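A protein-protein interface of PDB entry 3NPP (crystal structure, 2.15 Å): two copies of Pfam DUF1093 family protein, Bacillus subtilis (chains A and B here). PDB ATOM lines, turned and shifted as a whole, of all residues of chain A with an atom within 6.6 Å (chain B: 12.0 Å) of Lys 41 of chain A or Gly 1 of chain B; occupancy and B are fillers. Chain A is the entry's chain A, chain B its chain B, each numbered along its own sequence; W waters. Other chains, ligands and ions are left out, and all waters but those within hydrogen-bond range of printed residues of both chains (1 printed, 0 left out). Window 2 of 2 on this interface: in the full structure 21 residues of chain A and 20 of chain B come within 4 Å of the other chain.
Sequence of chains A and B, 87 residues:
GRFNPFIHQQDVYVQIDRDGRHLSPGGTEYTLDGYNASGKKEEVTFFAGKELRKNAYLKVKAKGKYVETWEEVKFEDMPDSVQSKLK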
ATOM      1  N   ASP A  33     -19.896   5.006 -20.917  1.00  0.00           N
ATOM      2  CA  ASP A  33     -19.626   3.688 -21.467  1.00  0.00           C
ATOM      3  C   ASP A  33     -18.228   3.663 -21.990  1.00  0.00           C
ATOM      4  O   ASP A  33     -17.776   4.631 -22.583  1.00  0.00           O
ATOM      5  CB  ASP A  33     -20.600   3.327 -22.596  1.00  0.00           C
ATOM      6  CG  ASP A  33     -22.009   3.084 -22.094  1.00  0.00           C
ATOM      7  OD1 ASP A  33     -22.211   2.748 -20.894  1.00  0.00           O
ATOM      8  OD2 ASP A  33     -22.915   3.220 -22.917  1.00  0.00           O
ATOM      9  N   GLY A  34     -17.551   2.542 -21.810  1.00  0.00           N
ATOM     10  CA  GLY A  34     -16.150   2.416 -22.210  1.00  0.00           C
ATOM     11  C   GLY A  34     -15.787   0.997 -22.537  1.00  0.00           C
ATOM     12  O   GLY A  34     -16.662   0.145 -22.640  1.00  0.00           O
ATOM     13  N   TYR A  35     -14.501   0.757 -22.755  1.00  0.00           N
ATOM     14  CA  TYR A  35     -14.016  -0.560 -23.114  1.00  0.00           C
ATOM     15  C   TYR A  35     -12.788  -0.862 -22.300  1.00  0.00           C
ATOM     16  O   TYR A  35     -11.941   0.023 -22.118  1.00  0.00           O
ATOM     17  CB  TYR A  35     -13.759  -0.640 -24.638  1.00  0.00           C
ATOM     18  CG  TYR A  35     -15.064  -0.467 -25.429  1.00  0.00           C
ATOM     19  CD1 TYR A  35     -15.549   0.808 -25.741  1.00  0.00           C
ATOM     20  CD2 TYR A  35     -15.877  -1.570 -25.740  1.00  0.00           C
ATOM     21  CE1 TYR A  35     -16.785   0.986 -26.383  1.00  0.00           C
ATOM     22  CE2 TYR A  35     -17.120  -1.403 -26.420  1.00  0.00           C
ATOM     23  CZ  TYR A  35     -17.555  -0.117 -26.719  1.00  0.00           C
ATOM     24  OH  TYR A  35     -18.750   0.091 -27.353  1.00  0.00           O
ATOM     25  N   ASN A  36     -12.669  -2.096 -21.800  1.00  0.00           N
ATOM     26  CA  ASN A  36     -11.457  -2.483 -21.080  1.00  0.00           C
ATOM     27  C   ASN A  36     -10.344  -2.822 -22.063  1.00  0.00           C
ATOM     28  O   ASN A  36     -10.541  -2.651 -23.294  1.00  0.00           O
ATOM     29  CB  ASN A  36     -11.740  -3.547 -19.991  1.00  0.00           C
ATOM     30  CG  ASN A  36     -11.898  -4.977 -20.532  1.00  0.00           C
ATOM     31  OD1 ASN A  36     -11.927  -5.242 -21.749  1.00  0.00           O
ATOM     32  ND2 ASN A  36     -11.996  -5.916 -19.592  1.00  0.00           N
ATOM     33  N   GLY A  39     -11.108  -5.039 -24.863  1.00  0.00           N
ATOM     34  CA  GLY A  39     -12.235  -4.604 -25.689  1.00  0.00           C
ATOM     35  C   GLY A  39     -13.632  -4.950 -25.189  1.00  0.00           C
ATOM     36  O   GLY A  39     -14.589  -4.822 -25.934  1.00  0.00           O
ATOM     37  N   LYS A  40     -13.769  -5.373 -23.935  1.00  0.00           N
ATOM     38  CA  LYS A  40     -15.083  -5.694 -23.386  1.00  0.00           C
ATOM     39  C   LYS A  40     -15.804  -4.399 -23.018  1.00  0.00           C
ATOM     40  O   LYS A  40     -15.199  -3.521 -22.438  1.00  0.00           O
ATOM     41  CB  LYS A  40     -14.922  -6.586 -22.167  1.00  0.00           C
ATOM     42  CG  LYS A  40     -16.236  -7.048 -21.576  1.00  0.00           C
ATOM     43  CD  LYS A  40     -16.063  -8.259 -20.679  1.00  0.00           C
ATOM     44  CE  LYS A  40     -17.423  -8.792 -20.247  1.00  0.00           C
ATOM     45  NZ  LYS A  40     -17.277 -10.108 -19.570  1.00  0.00           N
ATOM     46  N   LYS A  41     -17.090  -4.294 -23.329  1.00  0.00           N
ATOM     47  CA  LYS A  41     -17.890  -3.091 -22.986  1.00  0.00           C
ATOM     48  C   LYS A  41     -18.108  -2.987 -21.466  1.00  0.00           C
ATOM     49  O   LYS A  41     -18.358  -4.001 -20.805  1.00  0.00           O
ATOM     50  CB  LYS A  41     -19.256  -3.091 -23.721  1.00  0.00           C
ATOM     51  CG  LYS A  41     -19.926  -1.690 -23.820  1.00  0.00           C
ATOM     52  CD  LYS A  41     -21.086  -1.707 -24.873  1.00  0.00           C
ATOM     53  CE  LYS A  41     -21.673  -0.287 -25.141  1.00  0.00           C
ATOM     54  NZ  LYS A  41     -22.606  -0.290 -26.323  1.00  0.00           N
ATOM     55  N   GLU A  42     -17.962  -1.764 -20.932  1.00  0.00           N
ATOM     56  CA  GLU A  42     -18.074  -1.472 -19.484  1.00  0.00           C
ATOM     57  C   GLU A  42     -18.819  -0.158 -19.246  1.00  0.00           C
ATOM     58  O   GLU A  42     -18.846   0.692 -20.104  1.00  0.00           O
ATOM     59  CB  GLU A  42     -16.687  -1.310 -18.825  1.00  0.00           C
ATOM     60  CG  GLU A  42     -15.615  -2.261 -19.230  1.00  0.00           C
ATOM     61  CD  GLU A  42     -15.845  -3.697 -18.786  1.00  0.00           C
ATOM     62  OE1 GLU A  42     -16.882  -4.023 -18.135  1.00  0.00           O
ATOM     63  OE2 GLU A  42     -14.933  -4.499 -19.049  1.00  0.00           O
ATOM     64  N   GLU A  43     -19.369   0.013 -18.061  1.00  0.00           N
ATOM     65  CA  GLU A  43     -19.854   1.313 -17.596  1.00  0.00           C
ATOM     66  C   GLU A  43     -18.985   1.701 -16.438  1.00  0.00           C
ATOM     67  O   GLU A  43     -18.777   0.905 -15.543  1.00  0.00           O
ATOM     68  CB  GLU A  43     -21.318   1.220 -17.174  1.00  0.00           C
ATOM     69  CG  GLU A  43     -21.981   2.611 -16.826  1.00  0.00           C
ATOM     70  CD  GLU A  43     -23.229   2.457 -15.947  1.00  0.00           C
ATOM     71  OE1 GLU A  43     -24.304   2.163 -16.506  1.00  0.00           O
ATOM     72  OE2 GLU A  43     -23.115   2.606 -14.688  1.00  0.00           O
ATOM     73  N   VAL A  44     -18.474   2.927 -16.450  1.00  0.00           N
ATOM     74  CA  VAL A  44     -17.606   3.395 -15.387  1.00  0.00           C
ATOM     75  C   VAL A  44     -18.120   4.744 -14.852  1.00  0.00           C
ATOM     76  O   VAL A  44     -18.452   5.627 -15.626  1.00  0.00           O
ATOM     77  CB  VAL A  44     -16.127   3.455 -15.869  1.00  0.00           C
ATOM     78  CG1 VAL A  44     -15.948   4.358 -17.100  1.00  0.00           C
ATOM     79  CG2 VAL A  44     -15.209   3.855 -14.726  1.00  0.00           C
ATOM     80  N   LYS A  85     -13.794   0.599 -31.483  1.00  0.00           N
ATOM     81  CA  LYS A  85     -15.093   0.779 -30.813  1.00  0.00           C
ATOM     82  C   LYS A  85     -15.400   2.221 -30.410  1.00  0.00           C
ATOM     83  O   LYS A  85     -16.550   2.606 -30.391  1.00  0.00           O
ATOM     84  CB  LYS A  85     -15.213  -0.162 -29.600  1.00  0.00           C
ATOM     85  CG  LYS A  85     -15.698  -1.594 -29.987  1.00  0.00           C
ATOM     86  CD  LYS A  85     -15.039  -2.679 -29.137  1.00  0.00           C
ATOM     87  CE  LYS A  85     -15.419  -4.103 -29.598  1.00  0.00           C
ATOM     88  NZ  LYS A  85     -14.761  -5.133 -28.701  1.00  0.00           N
ATOM     89  N   GLY B   1     -19.496  -4.962 -17.703  1.00  0.00           N
ATOM     90  CA  GLY B   1     -19.612  -4.757 -16.226  1.00  0.00           C
ATOM     91  C   GLY B   1     -19.559  -3.307 -15.789  1.00  0.00           C
ATOM     92  O   GLY B   1     -19.285  -2.421 -16.585  1.00  0.00           O
ATOM     93  N   ARG B   2     -19.779  -3.088 -14.496  1.00  0.00           N
ATOM     94  CA  ARG B   2     -19.928  -1.745 -13.911  1.00  0.00           C
ATOM     95  C   ARG B   2     -18.852  -1.483 -12.869  1.00  0.00           C
ATOM     96  O   ARG B   2     -18.580  -2.332 -12.025  1.00  0.00           O
ATOM     97  CB  ARG B   2     -21.314  -1.570 -13.296  1.00  0.00           C
ATOM     98  CG  ARG B   2     -22.443  -1.826 -14.316  1.00  0.00           C
ATOM     99  CD  ARG B   2     -23.797  -1.230 -13.886  1.00  0.00           C
ATOM    100  NE  ARG B   2     -24.454  -1.957 -12.788  1.00  0.00           N
ATOM    101  CZ  ARG B   2     -24.329  -1.708 -11.460  1.00  0.00           C
ATOM    102  NH1 ARG B   2     -23.531  -0.737 -10.968  1.00  0.00           N
ATOM    103  NH2 ARG B   2     -25.018  -2.462 -10.585  1.00  0.00           N
ATOM    104  N   PHE B   3     -18.241  -0.308 -12.957  1.00  0.00           N
ATOM    105  CA  PHE B   3     -17.156   0.109 -12.084  1.00  0.00           C
ATOM    106  C   PHE B   3     -17.558   1.417 -11.419  1.00  0.00           C
ATOM    107  O   PHE B   3     -18.238   2.245 -12.027  1.00  0.00           O
ATOM    108  CB  PHE B   3     -15.863   0.312 -12.881  1.00  0.00           C
ATOM    109  CG  PHE B   3     -15.359  -0.939 -13.546  1.00  0.00           C
ATOM    110  CD1 PHE B   3     -15.927  -1.383 -14.721  1.00  0.00           C
ATOM    111  CD2 PHE B   3     -14.345  -1.696 -12.979  1.00  0.00           C
ATOM    112  CE1 PHE B   3     -15.491  -2.546 -15.323  1.00  0.00           C
ATOM    113  CE2 PHE B   3     -13.923  -2.886 -13.582  1.00  0.00           C
ATOM    114  CZ  PHE B   3     -14.491  -3.296 -14.760  1.00  0.00           C
ATOM    115  N   ASN B   4     -17.133   1.602 -10.174  1.00  0.00           N
ATOM    116  CA  ASN B   4     -17.363   2.857  -9.450  1.00  0.00           C
ATOM    117  C   ASN B   4     -16.349   3.018  -8.325  1.00  0.00           C
ATOM    118  O   ASN B   4     -15.647   2.063  -8.021  1.00  0.00           O
ATOM    119  CB  ASN B   4     -18.821   2.925  -8.963  1.00  0.00           C
ATOM    120  CG  ASN B   4     -19.150   1.858  -7.984  1.00  0.00           C
ATOM    121  OD1 ASN B   4     -18.554   1.776  -6.932  1.00  0.00           O
ATOM    122  ND2 ASN B   4     -20.142   1.058  -8.302  1.00  0.00           N
ATOM    123  N   PRO B   5     -16.277   4.215  -7.689  1.00  0.00           N
ATOM    124  CA  PRO B   5     -15.357   4.395  -6.567  1.00  0.00           C
ATOM    125  C   PRO B   5     -15.998   4.168  -5.171  1.00  0.00           C
ATOM    126  O   PRO B   5     -15.459   4.632  -4.196  1.00  0.00           O
ATOM    127  CB  PRO B   5     -14.889   5.850  -6.766  1.00  0.00           C
ATOM    128  CG  PRO B   5     -16.014   6.531  -7.450  1.00  0.00           C
ATOM    129  CD  PRO B   5     -16.978   5.486  -7.961  1.00  0.00           C
ATOM    130  N   LYS B  65     -14.186  -7.480  -1.995  1.00  0.00           N
ATOM    131  CA  LYS B  65     -13.748  -8.872  -1.752  1.00  0.00           C
ATOM    132  C   LYS B  65     -12.214  -9.059  -1.590  1.00  0.00           C
ATOM    133  O   LYS B  65     -11.768 -10.190  -1.466  1.00  0.00           O
ATOM    134  CB  LYS B  65     -14.285  -9.806  -2.866  1.00  0.00           C
ATOM    135  CG  LYS B  65     -13.830  -9.451  -4.324  1.00  0.00           C
ATOM    136  CD  LYS B  65     -14.070 -10.601  -5.299  1.00  0.00           C
ATOM    137  CE  LYS B  65     -14.011 -10.134  -6.715  1.00  0.00           C
ATOM    138  NZ  LYS B  65     -14.467 -11.201  -7.643  1.00  0.00           N
HETATM  139  O   HOH W   1     -20.837   2.835 -13.322  1.00  0.00           O
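The backbone carbonyl oxygen (O) of Glu 43 of chain A sits at hydrogen-bond distance from the backbone NH (N) of Phe 3 of chain B (2.9 Å). The backbone carbonyl oxygen of Lys 41 of chain A sits at hydrogen-bond distance from the backbone NH of Gly 1 of chain B (3.4 Å). The side-chain carboxylate of Glu 42 of chain A is in hydrogen-bond range of the backbone NH of Gly 1 of chain B, 2.8 Å away. The backbone NH (N) of Glu 43 of chain A lies within hydrogen-bond range of the backbone carbonyl oxygen (O) of Gly 1 of chain B.
OE2 of Glu 42 of chain A lies within hydrogen-bond range of ND2 of Asn 36 of chain A (3.3 Å). N of Gly 34 of chain A is in hydrogen-bond range of O of Glu 42 of chain A, at 2.8 Å.
Among the printed residues, pairs that only touch across the chains: Glu 43 of chain A with Arg 2 of chain B, Glu 42 of chain A with Phe 3 of chain B and Val 44 of chain A with Phe 3 of chain B.
Of chain B, only Gly 1 (3.4 Å) comes within 4 Å of Lys 41 of chain A. Gly 1 of chain B touches just these residues of chain A: Lys 41 (3.4 Å), Glu 42 (2.8 Å) and Glu 43 (2.8 Å). Asp 33 of chain A touches none of the printed residues of chain B. No residue of chain B comes within 4 Å of Gly 34 of chain A. No residue of chain B comes within 4 Å of Asn 36 of chain A. No residue of chain B comes within 4 Å of Gly 39 of chain A. No residue of chain B comes within 4 Å of Lys 40 of chain A. Glu 43 of chain A touches just these residues of chain B: Gly 1, Arg 2 and Phe 3. Printed residues of chain A within 4 Å of Arg 2 of chain B: Glu 43. Printed residues of chain B within 4 Å of Val 44 of chain A: Phe 3 (3.6 Å). Of the printed residues of chain A, Phe 3 of chain B touches Glu 42, Glu 43 and Val 44. The nearest residue of chain A that does not touch Gly 1 of chain B is Lys 40 of chain A (5.0 Å).
Along chain B the printed residues that touch a printed residue of chain A span positions 1 to 3. Of the 11 printed residues of chain A, 4 touch a printed residue of chain B. Among the printed residues, 7 pairs touch across the chains. Among the printed residues, no Asp or Glu carboxylate lies within 4 Å of a Lys or Arg side-chain nitrogen of the other chain.
No position is printed for both chains. Of the 7 pairs that touch across the chains among the printed residues, none has its exchanged pair printed and touching as well.
Water W1 lies within hydrogen-bond range of the side-chain carboxylate of Glu 43 of chain A (2.7 Å) and the backbone carbonyl oxygen of Phe 3 of chain B (3.0 Å).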
